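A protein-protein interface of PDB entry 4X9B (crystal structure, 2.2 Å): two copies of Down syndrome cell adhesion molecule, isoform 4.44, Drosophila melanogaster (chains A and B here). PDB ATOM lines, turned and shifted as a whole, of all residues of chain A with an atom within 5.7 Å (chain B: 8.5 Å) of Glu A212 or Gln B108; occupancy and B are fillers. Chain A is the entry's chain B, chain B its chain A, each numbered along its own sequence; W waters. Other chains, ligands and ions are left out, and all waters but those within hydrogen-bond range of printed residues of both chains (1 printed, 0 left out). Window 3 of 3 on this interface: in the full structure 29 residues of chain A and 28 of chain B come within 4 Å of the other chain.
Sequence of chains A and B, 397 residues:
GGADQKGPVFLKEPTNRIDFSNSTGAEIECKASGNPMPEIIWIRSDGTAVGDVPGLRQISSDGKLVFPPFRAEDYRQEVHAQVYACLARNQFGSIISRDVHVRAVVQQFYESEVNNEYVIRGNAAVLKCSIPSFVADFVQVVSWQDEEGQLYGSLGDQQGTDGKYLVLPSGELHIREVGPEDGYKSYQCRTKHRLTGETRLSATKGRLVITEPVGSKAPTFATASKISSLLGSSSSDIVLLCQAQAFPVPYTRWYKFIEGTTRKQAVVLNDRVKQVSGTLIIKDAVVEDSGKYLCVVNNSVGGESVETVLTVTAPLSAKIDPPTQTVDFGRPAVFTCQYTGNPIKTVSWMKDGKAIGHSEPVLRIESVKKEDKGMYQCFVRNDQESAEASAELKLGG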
ATOM      1  N   ILE A 120     -18.012  10.687 -21.758  1.00  0.00           N
ATOM      2  CA  ILE A 120     -18.750  10.721 -20.505  1.00  0.00           C
ATOM      3  C   ILE A 120     -19.238   9.309 -20.207  1.00  0.00           C
ATOM      4  O   ILE A 120     -19.765   8.636 -21.086  1.00  0.00           O
ATOM      5  CB  ILE A 120     -19.944  11.689 -20.567  1.00  0.00           C
ATOM      6  CG1 ILE A 120     -19.475  13.091 -20.959  1.00  0.00           C
ATOM      7  CG2 ILE A 120     -20.667  11.733 -19.227  1.00  0.00           C
ATOM      8  CD1 ILE A 120     -20.604  14.048 -21.337  1.00  0.00           C
ATOM      9  N   ARG A 121     -19.056   8.865 -18.969  1.00  0.00           N
ATOM     10  CA  ARG A 121     -19.454   7.518 -18.568  1.00  0.00           C
ATOM     11  C   ARG A 121     -20.911   7.214 -18.925  1.00  0.00           C
ATOM     12  O   ARG A 121     -21.801   8.047 -18.733  1.00  0.00           O
ATOM     13  CB  ARG A 121     -19.246   7.336 -17.062  1.00  0.00           C
ATOM     14  CG  ARG A 121     -19.359   5.892 -16.600  1.00  0.00           C
ATOM     15  CD  ARG A 121     -20.393   5.744 -15.509  1.00  0.00           C
ATOM     16  NE  ARG A 121     -20.034   6.498 -14.308  1.00  0.00           N
ATOM     17  CZ  ARG A 121     -20.877   7.244 -13.594  1.00  0.00           C
ATOM     18  NH1 ARG A 121     -22.157   7.363 -13.938  1.00  0.00           N
ATOM     19  NH2 ARG A 121     -20.435   7.887 -12.523  1.00  0.00           N
ATOM     20  N   PRO A 180     -15.881   2.360 -16.016  1.00  0.00           N
ATOM     21  CA  PRO A 180     -14.515   2.489 -15.495  1.00  0.00           C
ATOM     22  C   PRO A 180     -13.549   1.413 -16.004  1.00  0.00           C
ATOM     23  O   PRO A 180     -12.388   1.724 -16.284  1.00  0.00           O
ATOM     24  CB  PRO A 180     -14.715   2.370 -13.983  1.00  0.00           C
ATOM     25  CG  PRO A 180     -16.089   2.897 -13.752  1.00  0.00           C
ATOM     26  CD  PRO A 180     -16.891   2.479 -14.949  1.00  0.00           C
ATOM     27  N   ILE A 210     -12.300   8.650 -19.261  1.00  0.00           N
ATOM     28  CA  ILE A 210     -13.714   8.719 -18.916  1.00  0.00           C
ATOM     29  C   ILE A 210     -13.976   9.831 -17.907  1.00  0.00           C
ATOM     30  O   ILE A 210     -13.380   9.867 -16.834  1.00  0.00           O
ATOM     31  CB  ILE A 210     -14.206   7.379 -18.357  1.00  0.00           C
ATOM     32  CG1 ILE A 210     -13.928   6.251 -19.356  1.00  0.00           C
ATOM     33  CG2 ILE A 210     -15.695   7.435 -18.049  1.00  0.00           C
ATOM     34  CD1 ILE A 210     -13.926   4.882 -18.726  1.00  0.00           C
ATOM     35  N   THR A 211     -14.866  10.745 -18.275  1.00  0.00           N
ATOM     36  CA  THR A 211     -15.284  11.827 -17.395  1.00  0.00           C
ATOM     37  C   THR A 211     -16.529  11.416 -16.624  1.00  0.00           C
ATOM     38  O   THR A 211     -17.498  10.913 -17.203  1.00  0.00           O
ATOM     39  CB  THR A 211     -15.567  13.123 -18.192  1.00  0.00           C
ATOM     40  OG1 THR A 211     -14.343  13.621 -18.738  1.00  0.00           O
ATOM     41  CG2 THR A 211     -16.182  14.202 -17.309  1.00  0.00           C
ATOM     42  N   GLU A 212     -16.495  11.632 -15.314  1.00  0.00           N
ATOM     43  CA  GLU A 212     -17.640  11.344 -14.463  1.00  0.00           C
ATOM     44  C   GLU A 212     -18.666  12.464 -14.607  1.00  0.00           C
ATOM     45  O   GLU A 212     -18.336  13.632 -14.411  1.00  0.00           O
ATOM     46  CB  GLU A 212     -17.209  11.200 -13.000  1.00  0.00           C
ATOM     47  CG  GLU A 212     -16.310   9.997 -12.723  1.00  0.00           C
ATOM     48  CD  GLU A 212     -16.986   8.671 -13.038  1.00  0.00           C
ATOM     49  OE1 GLU A 212     -18.197   8.539 -12.759  1.00  0.00           O
ATOM     50  OE2 GLU A 212     -16.307   7.763 -13.569  1.00  0.00           O
ATOM     51  N   PRO A 213     -19.914  12.121 -14.962  1.00  0.00           N
ATOM     52  CA  PRO A 213     -20.913  13.183 -15.114  1.00  0.00           C
ATOM     53  C   PRO A 213     -21.181  13.917 -13.805  1.00  0.00           C
ATOM     54  O   PRO A 213     -21.420  13.276 -12.781  1.00  0.00           O
ATOM     55  CB  PRO A 213     -22.160  12.427 -15.582  1.00  0.00           C
ATOM     56  CG  PRO A 213     -21.972  11.045 -15.070  1.00  0.00           C
ATOM     57  CD  PRO A 213     -20.503  10.784 -15.153  1.00  0.00           C
ATOM     58  N   VAL A 214     -21.146  15.245 -13.844  1.00  0.00           N
ATOM     59  CA  VAL A 214     -21.423  16.048 -12.664  1.00  0.00           C
ATOM     60  C   VAL A 214     -22.768  16.759 -12.821  1.00  0.00           C
ATOM     61  O   VAL A 214     -23.770  16.368 -12.216  1.00  0.00           O
ATOM     62  CB  VAL A 214     -20.313  17.075 -12.424  1.00  0.00           C
ATOM     63  CG1 VAL A 214     -20.555  17.814 -11.125  1.00  0.00           C
ATOM     64  CG2 VAL A 214     -18.961  16.389 -12.392  1.00  0.00           C
ATOM     65  N   LYS A 217     -25.524  17.840 -19.417  1.00  0.00           N
ATOM     66  CA  LYS A 217     -25.047  18.302 -20.716  1.00  0.00           C
ATOM     67  C   LYS A 217     -25.983  17.833 -21.820  1.00  0.00           C
ATOM     68  O   LYS A 217     -26.274  16.644 -21.934  1.00  0.00           O
ATOM     69  CB  LYS A 217     -23.629  17.782 -20.999  1.00  0.00           C
ATOM     70  CG  LYS A 217     -22.615  18.054 -19.900  1.00  0.00           C
ATOM     71  CD  LYS A 217     -22.554  16.917 -18.883  1.00  0.00           C
ATOM     72  CE  LYS A 217     -21.412  17.113 -17.900  1.00  0.00           C
ATOM     73  NZ  LYS A 217     -21.326  15.991 -16.932  1.00  0.00           N
ATOM     74  N   SER B  21     -19.895  29.432 -13.715  1.00  0.00           N
ATOM     75  CA  SER B  21     -19.338  28.433 -12.819  1.00  0.00           C
ATOM     76  C   SER B  21     -20.137  28.365 -11.527  1.00  0.00           C
ATOM     77  O   SER B  21     -20.612  29.380 -11.013  1.00  0.00           O
ATOM     78  CB  SER B  21     -17.876  28.745 -12.500  1.00  0.00           C
ATOM     79  OG  SER B  21     -17.356  27.800 -11.581  1.00  0.00           O
ATOM     80  N   ASN B  22     -20.275  27.158 -10.999  1.00  0.00           N
ATOM     81  CA  ASN B  22     -20.928  26.975  -9.711  1.00  0.00           C
ATOM     82  C   ASN B  22     -20.280  27.810  -8.599  1.00  0.00           C
ATOM     83  O   ASN B  22     -20.922  28.116  -7.598  1.00  0.00           O
ATOM     84  CB  ASN B  22     -20.903  25.498  -9.329  1.00  0.00           C
ATOM     85  CG  ASN B  22     -19.522  25.032  -8.969  1.00  0.00           C
ATOM     86  OD1 ASN B  22     -18.647  24.918  -9.833  1.00  0.00           O
ATOM     87  ND2 ASN B  22     -19.306  24.766  -7.682  1.00  0.00           N
ATOM     88  N   ALA B  72     -21.156  21.197  -5.924  1.00  0.00           N
ATOM     89  CA  ALA B  72     -21.466  20.250  -6.988  1.00  0.00           C
ATOM     90  C   ALA B  72     -22.586  19.316  -6.569  1.00  0.00           C
ATOM     91  O   ALA B  72     -23.404  18.909  -7.387  1.00  0.00           O
ATOM     92  CB  ALA B  72     -20.236  19.448  -7.359  1.00  0.00           C
ATOM     93  N   VAL B 105     -22.130  25.470 -14.763  1.00  0.00           N
ATOM     94  CA  VAL B 105     -21.082  24.513 -15.044  1.00  0.00           C
ATOM     95  C   VAL B 105     -20.294  24.239 -13.767  1.00  0.00           C
ATOM     96  O   VAL B 105     -19.664  25.130 -13.205  1.00  0.00           O
ATOM     97  CB  VAL B 105     -20.150  25.028 -16.150  1.00  0.00           C
ATOM     98  CG1 VAL B 105     -19.165  23.953 -16.553  1.00  0.00           C
ATOM     99  CG2 VAL B 105     -20.973  25.475 -17.359  1.00  0.00           C
ATOM    100  N   VAL B 106     -20.357  23.002 -13.295  1.00  0.00           N
ATOM    101  CA  VAL B 106     -19.589  22.612 -12.128  1.00  0.00           C
ATOM    102  C   VAL B 106     -18.135  22.442 -12.523  1.00  0.00           C
ATOM    103  O   VAL B 106     -17.826  21.761 -13.498  1.00  0.00           O
ATOM    104  CB  VAL B 106     -20.099  21.312 -11.514  1.00  0.00           C
ATOM    105  CG1 VAL B 106     -19.308  20.998 -10.251  1.00  0.00           C
ATOM    106  CG2 VAL B 106     -21.583  21.426 -11.207  1.00  0.00           C
ATOM    107  N   GLN B 107     -17.246  23.057 -11.758  1.00  0.00           N
ATOM    108  CA  GLN B 107     -15.832  22.999 -12.073  1.00  0.00           C
ATOM    109  C   GLN B 107     -15.382  21.543 -12.154  1.00  0.00           C
ATOM    110  O   GLN B 107     -15.626  20.754 -11.241  1.00  0.00           O
ATOM    111  CB  GLN B 107     -15.032  23.778 -11.031  1.00  0.00           C
ATOM    112  CG  GLN B 107     -15.276  25.287 -11.092  1.00  0.00           C
ATOM    113  CD  GLN B 107     -14.583  26.043  -9.973  1.00  0.00           C
ATOM    114  OE1 GLN B 107     -14.653  25.651  -8.805  1.00  0.00           O
ATOM    115  NE2 GLN B 107     -13.912  27.134 -10.323  1.00  0.00           N
ATOM    116  N   GLN B 108     -14.772  21.190 -13.285  1.00  0.00           N
ATOM    117  CA  GLN B 108     -14.285  19.834 -13.521  1.00  0.00           C
ATOM    118  C   GLN B 108     -13.060  19.847 -14.440  1.00  0.00           C
ATOM    119  O   GLN B 108     -13.028  20.596 -15.416  1.00  0.00           O
ATOM    120  CB  GLN B 108     -15.400  18.986 -14.132  1.00  0.00           C
ATOM    121  CG  GLN B 108     -15.071  17.515 -14.287  1.00  0.00           C
ATOM    122  CD  GLN B 108     -16.243  16.723 -14.829  1.00  0.00           C
ATOM    123  OE1 GLN B 108     -16.959  17.184 -15.721  1.00  0.00           O
ATOM    124  NE2 GLN B 108     -16.455  15.530 -14.286  1.00  0.00           N
ATOM    125  N   PHE B 109     -12.076  18.994 -14.155  1.00  0.00           N
ATOM    126  CA  PHE B 109     -10.857  18.949 -14.962  1.00  0.00           C
ATOM    127  C   PHE B 109     -11.144  18.353 -16.342  1.00  0.00           C
ATOM    128  O   PHE B 109     -12.109  17.603 -16.528  1.00  0.00           O
ATOM    129  CB  PHE B 109      -9.756  18.140 -14.261  1.00  0.00           C
ATOM    130  CG  PHE B 109      -9.278  18.745 -12.963  1.00  0.00           C
ATOM    131  CD1 PHE B 109      -8.465  19.868 -12.963  1.00  0.00           C
ATOM    132  CD2 PHE B 109      -9.629  18.179 -11.745  1.00  0.00           C
ATOM    133  CE1 PHE B 109      -8.024  20.426 -11.778  1.00  0.00           C
ATOM    134  CE2 PHE B 109      -9.190  18.731 -10.551  1.00  0.00           C
ATOM    135  CZ  PHE B 109      -8.386  19.857 -10.568  1.00  0.00           C
ATOM    136  N   TYR B 110     -10.299  18.708 -17.306  1.00  0.00           N
ATOM    137  CA  TYR B 110     -10.406  18.215 -18.679  1.00  0.00           C
ATOM    138  C   TYR B 110      -8.998  18.157 -19.269  1.00  0.00           C
ATOM    139  O   TYR B 110      -8.109  18.862 -18.790  1.00  0.00           O
ATOM    140  CB  TYR B 110     -11.312  19.128 -19.522  1.00  0.00           C
ATOM    141  CG  TYR B 110     -10.693  20.480 -19.792  1.00  0.00           C
ATOM    142  CD1 TYR B 110     -10.843  21.532 -18.895  1.00  0.00           C
ATOM    143  CD2 TYR B 110      -9.935  20.697 -20.933  1.00  0.00           C
ATOM    144  CE1 TYR B 110     -10.256  22.771 -19.136  1.00  0.00           C
ATOM    145  CE2 TYR B 110      -9.352  21.920 -21.184  1.00  0.00           C
ATOM    146  CZ  TYR B 110      -9.513  22.955 -20.285  1.00  0.00           C
ATOM    147  OH  TYR B 110      -8.921  24.173 -20.551  1.00  0.00           O
ATOM    148  N   GLU B 111      -8.791  17.334 -20.299  1.00  0.00           N
ATOM    149  CA  GLU B 111      -7.527  17.347 -21.042  1.00  0.00           C
ATOM    150  C   GLU B 111      -7.722  17.762 -22.499  1.00  0.00           C
ATOM    151  O   GLU B 111      -8.714  17.412 -23.131  1.00  0.00           O
ATOM    152  CB  GLU B 111      -6.851  15.977 -21.004  1.00  0.00           C
ATOM    153  CG  GLU B 111      -6.707  15.391 -19.606  1.00  0.00           C
ATOM    154  CD  GLU B 111      -5.954  16.301 -18.668  1.00  0.00           C
ATOM    155  OE1 GLU B 111      -6.288  16.332 -17.463  1.00  0.00           O
ATOM    156  OE2 GLU B 111      -5.022  16.996 -19.122  1.00  0.00           O
ATOM    157  N   PHE B 134     -17.684  17.943 -25.000  1.00  0.00           N
ATOM    158  CA  PHE B 134     -18.596  18.354 -23.935  1.00  0.00           C
ATOM    159  C   PHE B 134     -18.065  19.542 -23.141  1.00  0.00           C
ATOM    160  O   PHE B 134     -18.828  20.174 -22.421  1.00  0.00           O
ATOM    161  CB  PHE B 134     -18.945  17.191 -22.982  1.00  0.00           C
ATOM    162  CG  PHE B 134     -17.801  16.265 -22.651  1.00  0.00           C
ATOM    163  CD1 PHE B 134     -17.520  15.173 -23.458  1.00  0.00           C
ATOM    164  CD2 PHE B 134     -17.046  16.453 -21.505  1.00  0.00           C
ATOM    165  CE1 PHE B 134     -16.486  14.310 -23.151  1.00  0.00           C
ATOM    166  CE2 PHE B 134     -16.010  15.589 -21.191  1.00  0.00           C
ATOM    167  CZ  PHE B 134     -15.733  14.516 -22.017  1.00  0.00           C
ATOM    168  N   VAL B 135     -16.765  19.817 -23.212  1.00  0.00           N
ATOM    169  CA  VAL B 135     -16.238  21.084 -22.700  1.00  0.00           C
ATOM    170  C   VAL B 135     -15.968  22.126 -23.795  1.00  0.00           C
ATOM    171  O   VAL B 135     -15.575  23.254 -23.510  1.00  0.00           O
ATOM    172  CB  VAL B 135     -14.955  20.845 -21.886  1.00  0.00           C
ATOM    173  CG1 VAL B 135     -15.214  19.767 -20.845  1.00  0.00           C
ATOM    174  CG2 VAL B 135     -13.801  20.443 -22.772  1.00  0.00           C
ATOM    175  N   VAL B 139     -13.931  26.193 -23.790  1.00  0.00           N
ATOM    176  CA  VAL B 139     -12.474  26.059 -23.844  1.00  0.00           C
ATOM    177  C   VAL B 139     -11.929  26.596 -25.158  1.00  0.00           C
ATOM    178  O   VAL B 139     -12.267  26.088 -26.230  1.00  0.00           O
ATOM    179  CB  VAL B 139     -12.039  24.588 -23.670  1.00  0.00           C
ATOM    180  CG1 VAL B 139     -10.529  24.457 -23.741  1.00  0.00           C
ATOM    181  CG2 VAL B 139     -12.537  24.033 -22.337  1.00  0.00           C
ATOM    182  N   HIS B 193     -10.041  27.972 -20.054  1.00  0.00           N
ATOM    183  CA  HIS B 193     -11.459  27.837 -19.748  1.00  0.00           C
ATOM    184  C   HIS B 193     -12.037  29.222 -19.464  1.00  0.00           C
ATOM    185  O   HIS B 193     -11.529  29.938 -18.608  1.00  0.00           O
ATOM    186  CB  HIS B 193     -11.646  26.908 -18.550  1.00  0.00           C
ATOM    187  CG  HIS B 193     -13.035  26.373 -18.404  1.00  0.00           C
ATOM    188  ND1 HIS B 193     -14.111  27.172 -18.087  1.00  0.00           N
ATOM    189  CD2 HIS B 193     -13.522  25.117 -18.527  1.00  0.00           C
ATOM    190  CE1 HIS B 193     -15.204  26.431 -18.025  1.00  0.00           C
ATOM    191  NE2 HIS B 193     -14.874  25.179 -18.289  1.00  0.00           N
ATOM    192  N   THR B 196     -13.892  29.273 -15.474  1.00  0.00           N
ATOM    193  CA  THR B 196     -12.934  29.143 -14.382  1.00  0.00           C
ATOM    194  C   THR B 196     -11.726  30.063 -14.569  1.00  0.00           C
ATOM    195  O   THR B 196     -11.181  30.581 -13.598  1.00  0.00           O
ATOM    196  CB  THR B 196     -12.429  27.704 -14.246  1.00  0.00           C
ATOM    197  OG1 THR B 196     -11.503  27.420 -15.300  1.00  0.00           O
ATOM    198  CG2 THR B 196     -13.587  26.712 -14.300  1.00  0.00           C
ATOM    199  N   GLU B 198      -8.855  29.118 -15.852  1.00  0.00           N
ATOM    200  CA  GLU B 198      -7.634  28.328 -15.790  1.00  0.00           C
ATOM    201  C   GLU B 198      -7.029  28.144 -17.172  1.00  0.00           C
ATOM    202  O   GLU B 198      -7.755  28.060 -18.156  1.00  0.00           O
ATOM    203  CB  GLU B 198      -7.924  26.956 -15.178  1.00  0.00           C
ATOM    204  CG  GLU B 198      -8.704  26.038 -16.125  1.00  0.00           C
ATOM    205  CD  GLU B 198      -9.145  24.745 -15.475  1.00  0.00           C
ATOM    206  OE1 GLU B 198      -8.263  23.941 -15.100  1.00  0.00           O
ATOM    207  OE2 GLU B 198     -10.373  24.527 -15.355  1.00  0.00           O
ATOM    208  N   ARG B 200      -4.041  25.579 -19.235  1.00  0.00           N
ATOM    209  CA  ARG B 200      -3.201  24.390 -19.133  1.00  0.00           C
ATOM    210  C   ARG B 200      -2.697  23.952 -20.500  1.00  0.00           C
ATOM    211  O   ARG B 200      -3.352  24.189 -21.521  1.00  0.00           O
ATOM    212  CB  ARG B 200      -3.973  23.237 -18.477  1.00  0.00           C
ATOM    213  CG  ARG B 200      -5.037  22.586 -19.386  1.00  0.00           C
ATOM    214  CD  ARG B 200      -5.769  21.443 -18.683  1.00  0.00           C
ATOM    215  NE  ARG B 200      -6.941  21.897 -17.935  1.00  0.00           N
ATOM    216  CZ  ARG B 200      -7.571  21.175 -17.012  1.00  0.00           C
ATOM    217  NH1 ARG B 200      -7.142  19.955 -16.700  1.00  0.00           N
ATOM    218  NH2 ARG B 200      -8.629  21.677 -16.391  1.00  0.00           N
HETATM  219  O   HOH W   1     -13.632  16.602 -18.290  1.00  0.00           O
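CG1 of Ile A120 touches CD1 of Phe B134, 3.8 Å away.
CG2 of Thr A211 touches NE2 of Gln B108, 3.3 Å away.
OG1 of Thr A211 touches CE2 of Phe B134, 3.6 Å away.
Val B106 touches Val A214 (CG1 to CG1, 3.5 Å).
CG2 of Val A214 touches NE2 of Gln B108, at 3.3 Å.
No position is printed for both chains.
Of the 6 pairs that touch across the chains among the printed residues, none has its exchanged pair printed and touching as well.
Water W1 bridges O of Phe B109 (2.5 Å) and OG1 of Thr A211 (3.1 Å).
Of the printed residues of chain B, Ile A120 touches Phe B134.
Printed residues of chain B within 4 Å of Thr A211: Gln B108 and Phe B134.
Glu A212 touches just one residue of chain B: Gln B108 (2.7 Å).
Of the printed residues of chain B, Val A214 touches Val B106 and Gln B108.
Printed residues of chain A within 4 Å of Val B106: Val A214.
Gln B108 touches just these residues of chain A: Thr A211, Glu A212 and Val A214.
Of the printed residues of chain A, Phe B134 touches Ile A120 (3.8 Å) and Thr A211 (3.6 Å).
The nearest residue of chain B that does not touch Glu A212 is Phe B134 (7.1 Å).
The nearest residue of chain A that does not touch Gln B108 is Lys A217 (4.7 Å).
The side-chain amide nitrogen (NE2) of Gln B108 is in hydrogen-bond range of the backbone carbonyl oxygen (O) of Glu A212, 2.7 Å away.
N of Arg A121 lies within hydrogen-bond range of O of Thr A211, 3.1 Å away.
The guanidinium group (NE) of Arg A121 is in salt-bridge range of the side-chain carboxylate (OE1) of Glu A212, 3.2 Å away.
Of the 9 printed residues of chain A, 4 touch a printed residue of chain B.
Hydrophobic or aromatic side chains of chain A within 4 Å of the printed part of chain B: Ile A120 and Val A214.
Of the 17 printed residues of chain B, 3 touch a printed residue of chain A.
Hydrophobic or aromatic side chains of chain B that line the printed part of chain A: Val B106 and Phe B134.
Among the printed residues, no Asp or Glu carboxylate lies within 4 Å of a Lys or Arg side-chain nitrogen of the other chain.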
